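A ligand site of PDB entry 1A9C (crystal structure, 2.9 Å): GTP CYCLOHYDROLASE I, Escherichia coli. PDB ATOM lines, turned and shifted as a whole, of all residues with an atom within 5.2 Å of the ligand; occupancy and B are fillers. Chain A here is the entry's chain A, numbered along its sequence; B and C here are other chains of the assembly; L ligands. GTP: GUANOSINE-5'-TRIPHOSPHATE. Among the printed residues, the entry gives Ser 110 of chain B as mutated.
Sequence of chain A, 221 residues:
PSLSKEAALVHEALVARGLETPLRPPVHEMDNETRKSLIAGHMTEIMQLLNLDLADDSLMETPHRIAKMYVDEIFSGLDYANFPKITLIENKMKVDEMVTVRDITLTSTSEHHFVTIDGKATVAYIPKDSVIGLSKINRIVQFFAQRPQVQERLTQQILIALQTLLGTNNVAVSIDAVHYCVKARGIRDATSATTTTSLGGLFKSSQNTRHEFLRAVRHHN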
ATOM      1  N   LYS A  85      33.139 -34.479  13.844  1.00  0.00           N
ATOM      2  CA  LYS A  85      33.385 -33.346  14.716  1.00  0.00           C
ATOM      3  C   LYS A  85      32.007 -32.956  15.180  1.00  0.00           C
ATOM      4  O   LYS A  85      31.132 -32.659  14.360  1.00  0.00           O
ATOM      5  CB  LYS A  85      34.029 -32.195  13.939  1.00  0.00           C
ATOM      6  N   THR A  87      29.352 -30.523  17.124  1.00  0.00           N
ATOM      7  CA  THR A  87      29.171 -29.132  17.500  1.00  0.00           C
ATOM      8  C   THR A  87      27.811 -29.073  18.167  1.00  0.00           C
ATOM      9  O   THR A  87      26.833 -29.658  17.693  1.00  0.00           O
ATOM     10  CB  THR A  87      29.216 -28.169  16.306  1.00  0.00           C
ATOM     11  OG1 THR A  87      28.178 -28.487  15.381  1.00  0.00           O
ATOM     12  CG2 THR A  87      30.551 -28.281  15.608  1.00  0.00           C
ATOM     13  N   ILE A  89      25.126 -26.359  20.295  1.00  0.00           N
ATOM     14  CA  ILE A  89      24.820 -24.969  20.568  1.00  0.00           C
ATOM     15  C   ILE A  89      24.059 -24.986  21.879  1.00  0.00           C
ATOM     16  O   ILE A  89      23.316 -25.925  22.175  1.00  0.00           O
ATOM     17  CB  ILE A  89      24.005 -24.279  19.426  1.00  0.00           C
ATOM     18  CG1 ILE A  89      22.689 -25.001  19.146  1.00  0.00           C
ATOM     19  CG2 ILE A  89      24.834 -24.238  18.161  1.00  0.00           C
ATOM     20  CD1 ILE A  89      21.871 -24.392  18.008  1.00  0.00           C
ATOM     21  N   VAL A 131      21.731 -28.291  22.271  1.00  0.00           N
ATOM     22  CA  VAL A 131      21.050 -28.704  21.058  1.00  0.00           C
ATOM     23  C   VAL A 131      22.176 -29.113  20.121  1.00  0.00           C
ATOM     24  O   VAL A 131      23.088 -28.331  19.899  1.00  0.00           O
ATOM     25  CB  VAL A 131      20.259 -27.510  20.466  1.00  0.00           C
ATOM     26  CG1 VAL A 131      19.698 -27.856  19.115  1.00  0.00           C
ATOM     27  CG2 VAL A 131      19.115 -27.149  21.384  1.00  0.00           C
ATOM     28  N   ILE A 132      22.125 -30.322  19.562  1.00  0.00           N
ATOM     29  CA  ILE A 132      23.182 -30.783  18.655  1.00  0.00           C
ATOM     30  C   ILE A 132      22.919 -30.304  17.235  1.00  0.00           C
ATOM     31  O   ILE A 132      21.770 -30.086  16.856  1.00  0.00           O
ATOM     32  CB  ILE A 132      23.312 -32.332  18.696  1.00  0.00           C
ATOM     33  CG1 ILE A 132      24.584 -32.779  17.967  1.00  0.00           C
ATOM     34  CG2 ILE A 132      22.084 -32.977  18.096  1.00  0.00           C
ATOM     35  CD1 ILE A 132      24.937 -34.213  18.266  1.00  0.00           C
ATOM     36  N   GLY A 133      23.987 -30.101  16.481  1.00  0.00           N
ATOM     37  CA  GLY A 133      23.852 -29.653  15.108  1.00  0.00           C
ATOM     38  C   GLY A 133      23.172 -30.777  14.354  1.00  0.00           C
ATOM     39  O   GLY A 133      23.616 -31.922  14.433  1.00  0.00           O
ATOM     40  N   LEU A 134      22.124 -30.460  13.618  1.00  0.00           N
ATOM     41  CA  LEU A 134      21.375 -31.467  12.875  1.00  0.00           C
ATOM     42  C   LEU A 134      22.198 -32.465  12.090  1.00  0.00           C
ATOM     43  O   LEU A 134      22.048 -33.675  12.292  1.00  0.00           O
ATOM     44  CB  LEU A 134      20.352 -30.803  11.939  1.00  0.00           C
ATOM     45  CG  LEU A 134      19.209 -30.054  12.623  1.00  0.00           C
ATOM     46  CD1 LEU A 134      18.392 -29.336  11.567  1.00  0.00           C
ATOM     47  CD2 LEU A 134      18.342 -30.994  13.447  1.00  0.00           C
ATOM     48  N   SER A 135      23.114 -31.993  11.242  1.00  0.00           N
ATOM     49  CA  SER A 135      23.933 -32.901  10.442  1.00  0.00           C
ATOM     50  C   SER A 135      24.731 -33.886  11.266  1.00  0.00           C
ATOM     51  O   SER A 135      24.993 -34.989  10.792  1.00  0.00           O
ATOM     52  CB  SER A 135      24.888 -32.148   9.524  1.00  0.00           C
ATOM     53  OG  SER A 135      25.862 -31.435  10.277  1.00  0.00           O
ATOM     54  N   LYS A 136      25.088 -33.518  12.487  1.00  0.00           N
ATOM     55  CA  LYS A 136      25.882 -34.410  13.349  1.00  0.00           C
ATOM     56  C   LYS A 136      25.147 -35.716  13.649  1.00  0.00           C
ATOM     57  O   LYS A 136      25.771 -36.754  13.739  1.00  0.00           O
ATOM     58  CB  LYS A 136      26.273 -33.703  14.653  1.00  0.00           C
ATOM     59  CG  LYS A 136      26.940 -32.336  14.434  1.00  0.00           C
ATOM     60  CD  LYS A 136      28.087 -32.418  13.486  1.00  0.00           C
ATOM     61  CE  LYS A 136      28.662 -31.042  13.238  1.00  0.00           C
ATOM     62  NZ  LYS A 136      29.848 -31.058  12.333  1.00  0.00           N
ATOM     63  N   ARG A 139      25.708 -37.726  10.671  1.00  0.00           N
ATOM     64  CA  ARG A 139      27.115 -38.167  10.687  1.00  0.00           C
ATOM     65  C   ARG A 139      27.372 -39.310  11.648  1.00  0.00           C
ATOM     66  O   ARG A 139      28.009 -40.286  11.283  1.00  0.00           O
ATOM     67  CB  ARG A 139      28.064 -36.993  10.965  1.00  0.00           C
ATOM     68  CG  ARG A 139      27.870 -35.850   9.983  1.00  0.00           C
ATOM     69  CD  ARG A 139      29.040 -34.871   9.923  1.00  0.00           C
ATOM     70  NE  ARG A 139      29.802 -35.091   8.691  1.00  0.00           N
ATOM     71  CZ  ARG A 139      29.986 -34.179   7.732  1.00  0.00           C
ATOM     72  NH1 ARG A 139      29.471 -32.963   7.839  1.00  0.00           N
ATOM     73  NH2 ARG A 139      30.644 -34.493   6.634  1.00  0.00           N
ATOM     74  N   SER B 110      19.227 -21.078   6.946  1.00  0.00           N
ATOM     75  CA  SER B 110      19.945 -21.512   8.155  1.00  0.00           C
ATOM     76  C   SER B 110      21.011 -20.443   8.486  1.00  0.00           C
ATOM     77  O   SER B 110      21.752 -19.994   7.601  1.00  0.00           O
ATOM     78  CB  SER B 110      20.602 -22.865   7.933  1.00  0.00           C
ATOM     79  OG  SER B 110      21.535 -22.835   6.871  1.00  0.00           O
ATOM     80  N   HIS B 112      23.665 -20.863  10.228  1.00  0.00           N
ATOM     81  CA  HIS B 112      24.981 -21.506  10.226  1.00  0.00           C
ATOM     82  C   HIS B 112      25.713 -21.486   8.895  1.00  0.00           C
ATOM     83  O   HIS B 112      26.943 -21.431   8.909  1.00  0.00           O
ATOM     84  CB  HIS B 112      24.858 -22.957  10.689  1.00  0.00           C
ATOM     85  CG  HIS B 112      24.321 -23.099  12.071  1.00  0.00           C
ATOM     86  ND1 HIS B 112      25.102 -23.468  13.140  1.00  0.00           N
ATOM     87  CD2 HIS B 112      23.071 -22.904  12.571  1.00  0.00           C
ATOM     88  CE1 HIS B 112      24.367 -23.497  14.245  1.00  0.00           C
ATOM     89  NE2 HIS B 112      23.127 -23.163  13.917  1.00  0.00           N
ATOM     90  N   HIS B 113      25.004 -21.600   7.768  1.00  0.00           N
ATOM     91  CA  HIS B 113      25.631 -21.608   6.442  1.00  0.00           C
ATOM     92  C   HIS B 113      24.930 -20.686   5.475  1.00  0.00           C
ATOM     93  O   HIS B 113      25.338 -20.604   4.315  1.00  0.00           O
ATOM     94  CB  HIS B 113      25.612 -23.007   5.787  1.00  0.00           C
ATOM     95  CG  HIS B 113      26.400 -24.034   6.522  1.00  0.00           C
ATOM     96  ND1 HIS B 113      25.825 -24.903   7.423  1.00  0.00           N
ATOM     97  CD2 HIS B 113      27.722 -24.321   6.504  1.00  0.00           C
ATOM     98  CE1 HIS B 113      26.762 -25.681   7.941  1.00  0.00           C
ATOM     99  NE2 HIS B 113      27.920 -25.354   7.394  1.00  0.00           N
ATOM    100  N   ILE B 117      16.264 -23.500   3.782  1.00  0.00           N
ATOM    101  CA  ILE B 117      15.513 -24.385   4.688  1.00  0.00           C
ATOM    102  C   ILE B 117      14.129 -24.350   4.029  1.00  0.00           C
ATOM    103  O   ILE B 117      13.512 -23.285   3.913  1.00  0.00           O
ATOM    104  CB  ILE B 117      15.355 -23.826   6.112  1.00  0.00           C
ATOM    105  CG1 ILE B 117      16.679 -23.821   6.849  1.00  0.00           C
ATOM    106  CG2 ILE B 117      14.314 -24.636   6.886  1.00  0.00           C
ATOM    107  CD1 ILE B 117      16.549 -23.416   8.295  1.00  0.00           C
ATOM    108  N   GLN B 149      17.797 -18.395  10.546  1.00  0.00           N
ATOM    109  CA  GLN B 149      17.245 -19.207  11.611  1.00  0.00           C
ATOM    110  C   GLN B 149      17.902 -20.507  12.040  1.00  0.00           C
ATOM    111  O   GLN B 149      18.889 -20.968  11.467  1.00  0.00           O
ATOM    112  CB  GLN B 149      15.793 -19.527  11.261  1.00  0.00           C
ATOM    113  CG  GLN B 149      14.863 -18.373  11.403  1.00  0.00           C
ATOM    114  CD  GLN B 149      14.572 -18.010  12.839  1.00  0.00           C
ATOM    115  OE1 GLN B 149      15.267 -18.438  13.775  1.00  0.00           O
ATOM    116  NE2 GLN B 149      13.529 -17.219  13.045  1.00  0.00           N
ATOM    117  N   VAL B 150      17.340 -21.058  13.091  1.00  0.00           N
ATOM    118  CA  VAL B 150      17.715 -22.311  13.698  1.00  0.00           C
ATOM    119  C   VAL B 150      16.287 -22.792  13.919  1.00  0.00           C
ATOM    120  O   VAL B 150      15.531 -22.168  14.676  1.00  0.00           O
ATOM    121  CB  VAL B 150      18.418 -22.136  15.040  1.00  0.00           C
ATOM    122  CG1 VAL B 150      18.431 -23.428  15.809  1.00  0.00           C
ATOM    123  CG2 VAL B 150      19.827 -21.700  14.790  1.00  0.00           C
ATOM    124  N   GLN B 151      15.922 -23.865  13.239  1.00  0.00           N
ATOM    125  CA  GLN B 151      14.578 -24.410  13.317  1.00  0.00           C
ATOM    126  C   GLN B 151      14.008 -24.460  14.735  1.00  0.00           C
ATOM    127  O   GLN B 151      12.855 -24.093  14.953  1.00  0.00           O
ATOM    128  CB  GLN B 151      14.543 -25.780  12.657  1.00  0.00           C
ATOM    129  CG  GLN B 151      13.147 -26.334  12.540  1.00  0.00           C
ATOM    130  CD  GLN B 151      13.104 -27.636  11.781  1.00  0.00           C
ATOM    131  OE1 GLN B 151      13.952 -27.887  10.930  1.00  0.00           O
ATOM    132  NE2 GLN B 151      12.136 -28.464  12.085  1.00  0.00           N
ATOM    133  N   GLU B 152      14.828 -24.871  15.696  1.00  0.00           N
ATOM    134  CA  GLU B 152      14.409 -24.958  17.078  1.00  0.00           C
ATOM    135  C   GLU B 152      13.923 -23.604  17.617  1.00  0.00           C
ATOM    136  O   GLU B 152      12.943 -23.542  18.360  1.00  0.00           O
ATOM    137  CB  GLU B 152      15.562 -25.484  17.960  1.00  0.00           C
ATOM    138  CG  GLU B 152      15.905 -26.970  17.792  1.00  0.00           C
ATOM    139  CD  GLU B 152      16.959 -27.281  16.699  1.00  0.00           C
ATOM    140  OE1 GLU B 152      17.169 -26.481  15.771  1.00  0.00           O
ATOM    141  OE2 GLU B 152      17.570 -28.363  16.791  1.00  0.00           O
ATOM    142  N   HIS B 179      16.849 -29.233   5.365  1.00  0.00           N
ATOM    143  CA  HIS B 179      17.925 -28.265   5.383  1.00  0.00           C
ATOM    144  C   HIS B 179      18.894 -28.560   4.261  1.00  0.00           C
ATOM    145  O   HIS B 179      19.535 -29.620   4.236  1.00  0.00           O
ATOM    146  CB  HIS B 179      18.651 -28.289   6.719  1.00  0.00           C
ATOM    147  CG  HIS B 179      17.772 -27.947   7.881  1.00  0.00           C
ATOM    148  ND1 HIS B 179      17.956 -26.799   8.613  1.00  0.00           N
ATOM    149  CD2 HIS B 179      16.713 -28.585   8.422  1.00  0.00           C
ATOM    150  CE1 HIS B 179      17.037 -26.751   9.567  1.00  0.00           C
ATOM    151  NE2 HIS B 179      16.285 -27.826   9.473  1.00  0.00           N
ATOM    152  N   CYS B 181      21.624 -27.381   3.940  1.00  0.00           N
ATOM    153  CA  CYS B 181      23.002 -27.375   4.414  1.00  0.00           C
ATOM    154  C   CYS B 181      23.357 -28.788   4.950  1.00  0.00           C
ATOM    155  O   CYS B 181      24.447 -29.008   5.481  1.00  0.00           O
ATOM    156  CB  CYS B 181      23.238 -26.253   5.457  1.00  0.00           C
ATOM    157  SG  CYS B 181      22.505 -26.388   7.102  1.00  0.00           S
ATOM    158  N   VAL B 182      22.417 -29.730   4.787  1.00  0.00           N
ATOM    159  CA  VAL B 182      22.569 -31.122   5.193  1.00  0.00           C
ATOM    160  C   VAL B 182      22.438 -31.950   3.910  1.00  0.00           C
ATOM    161  O   VAL B 182      23.129 -32.952   3.702  1.00  0.00           O
ATOM    162  CB  VAL B 182      21.437 -31.570   6.165  1.00  0.00           C
ATOM    163  CG1 VAL B 182      21.496 -33.053   6.421  1.00  0.00           C
ATOM    164  CG2 VAL B 182      21.573 -30.876   7.475  1.00  0.00           C
ATOM    165  N   ARG B 185      25.081 -30.415   0.694  1.00  0.00           N
ATOM    166  CA  ARG B 185      26.507 -30.455   0.956  1.00  0.00           C
ATOM    167  C   ARG B 185      26.820 -31.079   2.319  1.00  0.00           C
ATOM    168  O   ARG B 185      25.909 -31.463   3.042  1.00  0.00           O
ATOM    169  CB  ARG B 185      27.050 -29.022   0.779  1.00  0.00           C
ATOM    170  CG  ARG B 185      27.721 -28.340   1.939  1.00  0.00           C
ATOM    171  CD  ARG B 185      26.815 -27.829   3.000  1.00  0.00           C
ATOM    172  NE  ARG B 185      27.671 -27.297   4.043  1.00  0.00           N
ATOM    173  CZ  ARG B 185      28.105 -27.989   5.100  1.00  0.00           C
ATOM    174  NH1 ARG B 185      27.768 -29.251   5.260  1.00  0.00           N
ATOM    175  NH2 ARG B 185      28.928 -27.435   5.974  1.00  0.00           N
ATOM    176  N   GLY B 186      28.094 -31.225   2.652  1.00  0.00           N
ATOM    177  CA  GLY B 186      28.484 -31.807   3.922  1.00  0.00           C
ATOM    178  C   GLY B 186      28.194 -33.285   3.901  1.00  0.00           C
ATOM    179  O   GLY B 186      28.785 -33.993   3.085  1.00  0.00           O
ATOM    180  N   ILE B 187      27.292 -33.758   4.759  1.00  0.00           N
ATOM    181  CA  ILE B 187      26.972 -35.184   4.758  1.00  0.00           C
ATOM    182  C   ILE B 187      26.070 -35.591   3.574  1.00  0.00           C
ATOM    183  O   ILE B 187      25.901 -36.785   3.291  1.00  0.00           O
ATOM    184  CB  ILE B 187      26.322 -35.632   6.051  1.00  0.00           C
ATOM    185  CG1 ILE B 187      26.387 -37.150   6.107  1.00  0.00           C
ATOM    186  CG2 ILE B 187      24.896 -35.114   6.161  1.00  0.00           C
ATOM    187  CD1 ILE B 187      25.928 -37.745   7.386  1.00  0.00           C
ATOM    188  N   GLU C  61      30.666 -18.391  14.260  1.00  0.00           N
ATOM    189  CA  GLU C  61      31.444 -19.082  13.246  1.00  0.00           C
ATOM    190  C   GLU C  61      30.879 -19.139  11.846  1.00  0.00           C
ATOM    191  O   GLU C  61      31.529 -19.692  10.948  1.00  0.00           O
ATOM    192  CB  GLU C  61      31.793 -20.476  13.715  1.00  0.00           C
ATOM    193  CG  GLU C  61      32.719 -20.479  14.905  1.00  0.00           C
ATOM    194  CD  GLU C  61      33.125 -21.874  15.313  1.00  0.00           C
ATOM    195  OE1 GLU C  61      33.807 -22.541  14.496  1.00  0.00           O
ATOM    196  OE2 GLU C  61      32.754 -22.298  16.431  1.00  0.00           O
ATOM    197  N   ARG C  65      32.249 -20.786   8.314  1.00  0.00           N
ATOM    198  CA  ARG C  65      31.508 -21.856   7.641  1.00  0.00           C
ATOM    199  C   ARG C  65      31.131 -21.502   6.207  1.00  0.00           C
ATOM    200  O   ARG C  65      31.220 -22.350   5.320  1.00  0.00           O
ATOM    201  CB  ARG C  65      30.242 -22.223   8.413  1.00  0.00           C
ATOM    202  CG  ARG C  65      30.547 -22.964   9.704  1.00  0.00           C
ATOM    203  CD  ARG C  65      29.291 -23.375  10.448  1.00  0.00           C
ATOM    204  NE  ARG C  65      28.572 -22.214  10.959  1.00  0.00           N
ATOM    205  CZ  ARG C  65      28.299 -22.017  12.243  1.00  0.00           C
ATOM    206  NH1 ARG C  65      28.680 -22.895  13.163  1.00  0.00           N
ATOM    207  NH2 ARG C  65      27.685 -20.912  12.613  1.00  0.00           N
ATOM    208  N   LYS C  68      34.365 -21.445   3.935  1.00  0.00           N
ATOM    209  CA  LYS C  68      34.755 -22.832   3.674  1.00  0.00           C
ATOM    210  C   LYS C  68      33.811 -23.450   2.644  1.00  0.00           C
ATOM    211  O   LYS C  68      34.260 -24.081   1.689  1.00  0.00           O
ATOM    212  CB  LYS C  68      34.709 -23.634   4.969  1.00  0.00           C
ATOM    213  CG  LYS C  68      34.777 -25.137   4.785  1.00  0.00           C
ATOM    214  CD  LYS C  68      34.132 -25.821   5.994  1.00  0.00           C
ATOM    215  CE  LYS C  68      33.889 -27.301   5.759  1.00  0.00           C
ATOM    216  NZ  LYS C  68      33.150 -27.915   6.919  1.00  0.00           N
ATOM    217  N   GLU C  73      33.333 -26.489  -0.718  1.00  0.00           N
ATOM    218  CA  GLU C  73      32.156 -27.253  -1.085  1.00  0.00           C
ATOM    219  C   GLU C  73      31.374 -26.798  -2.312  1.00  0.00           C
ATOM    220  O   GLU C  73      31.809 -27.038  -3.439  1.00  0.00           O
ATOM    221  CB  GLU C  73      31.239 -27.385   0.141  1.00  0.00           C
ATOM    222  CG  GLU C  73      31.951 -28.005   1.347  1.00  0.00           C
ATOM    223  CD  GLU C  73      31.152 -27.942   2.641  1.00  0.00           C
ATOM    224  OE1 GLU C  73      30.597 -26.871   2.974  1.00  0.00           O
ATOM    225  OE2 GLU C  73      31.091 -28.972   3.335  1.00  0.00           O
HETATM  226  PG  GTP L   1      28.570 -30.000   8.680  1.00  0.00           P
HETATM  227  O1G GTP L   1      29.635 -30.093   7.617  1.00  0.00           O
HETATM  228  O2G GTP L   1      28.468 -31.062   9.734  1.00  0.00           O
HETATM  229  O3G GTP L   1      27.155 -30.013   7.919  1.00  0.00           O
HETATM  230  O3B GTP L   1      28.661 -28.483   9.377  1.00  0.00           O
HETATM  231  PB  GTP L   1      30.009 -27.622   9.500  1.00  0.00           P
HETATM  232  O1B GTP L   1      31.017 -28.556   9.980  1.00  0.00           O
HETATM  233  O2B GTP L   1      30.371 -26.933   8.269  1.00  0.00           O
HETATM  234  O3A GTP L   1      29.742 -26.537  10.653  1.00  0.00           O
HETATM  235  PA  GTP L   1      29.670 -26.750  12.301  1.00  0.00           P
HETATM  236  O1A GTP L   1      30.342 -28.039  12.671  1.00  0.00           O
HETATM  237  O2A GTP L   1      29.836 -25.528  13.098  1.00  0.00           O
HETATM  238  O5' GTP L   1      28.159 -27.124  12.582  1.00  0.00           O
HETATM  239  C5' GTP L   1      26.981 -26.395  12.194  1.00  0.00           C
HETATM  240  C4' GTP L   1      25.896 -27.265  12.774  1.00  0.00           C
HETATM  241  O4' GTP L   1      24.530 -26.712  12.983  1.00  0.00           O
HETATM  242  C3' GTP L   1      25.771 -28.363  11.788  1.00  0.00           C
HETATM  243  O3' GTP L   1      25.763 -29.621  12.481  1.00  0.00           O
HETATM  244  C2' GTP L   1      24.532 -28.009  10.995  1.00  0.00           C
HETATM  245  O2' GTP L   1      23.899 -29.050  10.155  1.00  0.00           O
HETATM  246  C1' GTP L   1      23.711 -27.545  12.180  1.00  0.00           C
HETATM  247  N9  GTP L   1      22.509 -26.796  11.867  1.00  0.00           N
HETATM  248  C8  GTP L   1      22.157 -26.039  10.793  1.00  0.00           C
HETATM  249  N7  GTP L   1      20.958 -25.497  10.829  1.00  0.00           N
HETATM  250  C5  GTP L   1      20.488 -25.959  12.050  1.00  0.00           C
HETATM  251  C6  GTP L   1      19.248 -25.751  12.715  1.00  0.00           C
HETATM  252  O6  GTP L   1      18.294 -25.122  12.342  1.00  0.00           O
HETATM  253  N1  GTP L   1      19.168 -26.398  13.947  1.00  0.00           N
HETATM  254  C2  GTP L   1      20.189 -27.165  14.499  1.00  0.00           C
HETATM  255  N2  GTP L   1      20.006 -27.724  15.695  1.00  0.00           N
HETATM  256  N3  GTP L   1      21.341 -27.354  13.867  1.00  0.00           N
HETATM  257  C4  GTP L   1      21.437 -26.739  12.659  1.00  0.00           C
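Val 131 touches the ligand.
CA of Gly 133 touches O3' of the ligand, 3.2 Å away.
CB of Ser 110 of chain B touches N7 of the ligand, 3.9 Å away.
Val 150 of chain B touches the ligand.
His 179 of chain B touches the ligand.
SG of Cys 181 of chain B touches C8 of the ligand, at 3.7 Å.
Val 182 of chain B touches the ligand.
Hydrophobic or aromatic side chains within 4 Å of the ligand: Val 131, Leu 134, His 112 of chain B, His 113 of chain B, Val 150 of chain B, His 179 of chain B and Val 182 of chain B.
Along chain A the residues within 4 Å of the ligand span positions 87 to 139.
NZ of Lys 68 of chain C is in salt-bridge range of O2B of the ligand.
The guanidinium group (NH1) of Arg 65 of chain C is in salt-bridge range of an oxygen (O2A) of the ligand.
An oxygen (O2B) of the ligand is in hydrogen-bond range of a ring nitrogen (NE2) of His 113 of chain B.
The side-chain carboxylate (OE1) of Glu 152 of chain B lies within hydrogen-bond range of a nitrogen (N1) of the ligand.
A ring nitrogen (ND1) of His 112 of chain B lies within hydrogen-bond range of an oxygen (O4') of the ligand, at 3.3 Å.
The guanidinium group (NH1) of Arg 139 is in salt-bridge range of an oxygen (O2G) of the ligand (2.9 Å).
N of Ser 135 lies within hydrogen-bond range of O2' of the ligand (3.2 Å).
The backbone carbonyl oxygen (O) of Ile 132 lies within hydrogen-bond range of a nitrogen (N2) of the ligand (3.2 Å).
OG of Ser 135 lies within hydrogen-bond range of O2G of the ligand.
An oxygen (O2G) of the ligand lies within salt-bridge range of the side-chain amino group of Lys 136 (2.9 Å).
N of Leu 134 sits at hydrogen-bond distance from N3 of the ligand, 3.2 Å away.
The backbone NH (N) of Gln 151 of chain B sits at hydrogen-bond distance from an oxygen (O6) of the ligand.
The side-chain hydroxyl of Thr 87 is in hydrogen-bond range of an oxygen (O5') of the ligand, 3.1 Å away.
The guanidinium group of Arg 185 of chain B lies within salt-bridge range of an oxygen (O2B) of the ligand (2.8 Å).
The guanidinium group (NE) of Arg 185 of chain B is in salt-bridge range of the side-chain carboxylate (OE1) of Glu 73 of chain C, 3.1 Å away.
The guanidinium group of Arg 185 of chain B is in hydrogen-bond range of the backbone carbonyl oxygen of Cys 181 of chain B (3.3 Å).
The backbone NH of Val 131 sits at hydrogen-bond distance from the backbone carbonyl oxygen of Ile 89.
NZ of Lys 136 is in hydrogen-bond range of O of Lys 85 (2.9 Å).
The guanidinium group (NE) of Arg 65 of chain C sits at hydrogen-bond distance from the backbone carbonyl oxygen (O) of His 112 of chain B (2.7 Å).
OE1 of Gln 151 of chain B lies within hydrogen-bond range of NE2 of His 179 of chain B (2.8 Å).
The side-chain sulfur of Cys 181 of chain B lies close to a ring nitrogen (ND1) of His 113 of chain B (3.7 Å).
The side-chain sulfur of Cys 181 of chain B sits at hydrogen-bond distance from the side-chain hydroxyl of Ser 110 of chain B, 3.7 Å away.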
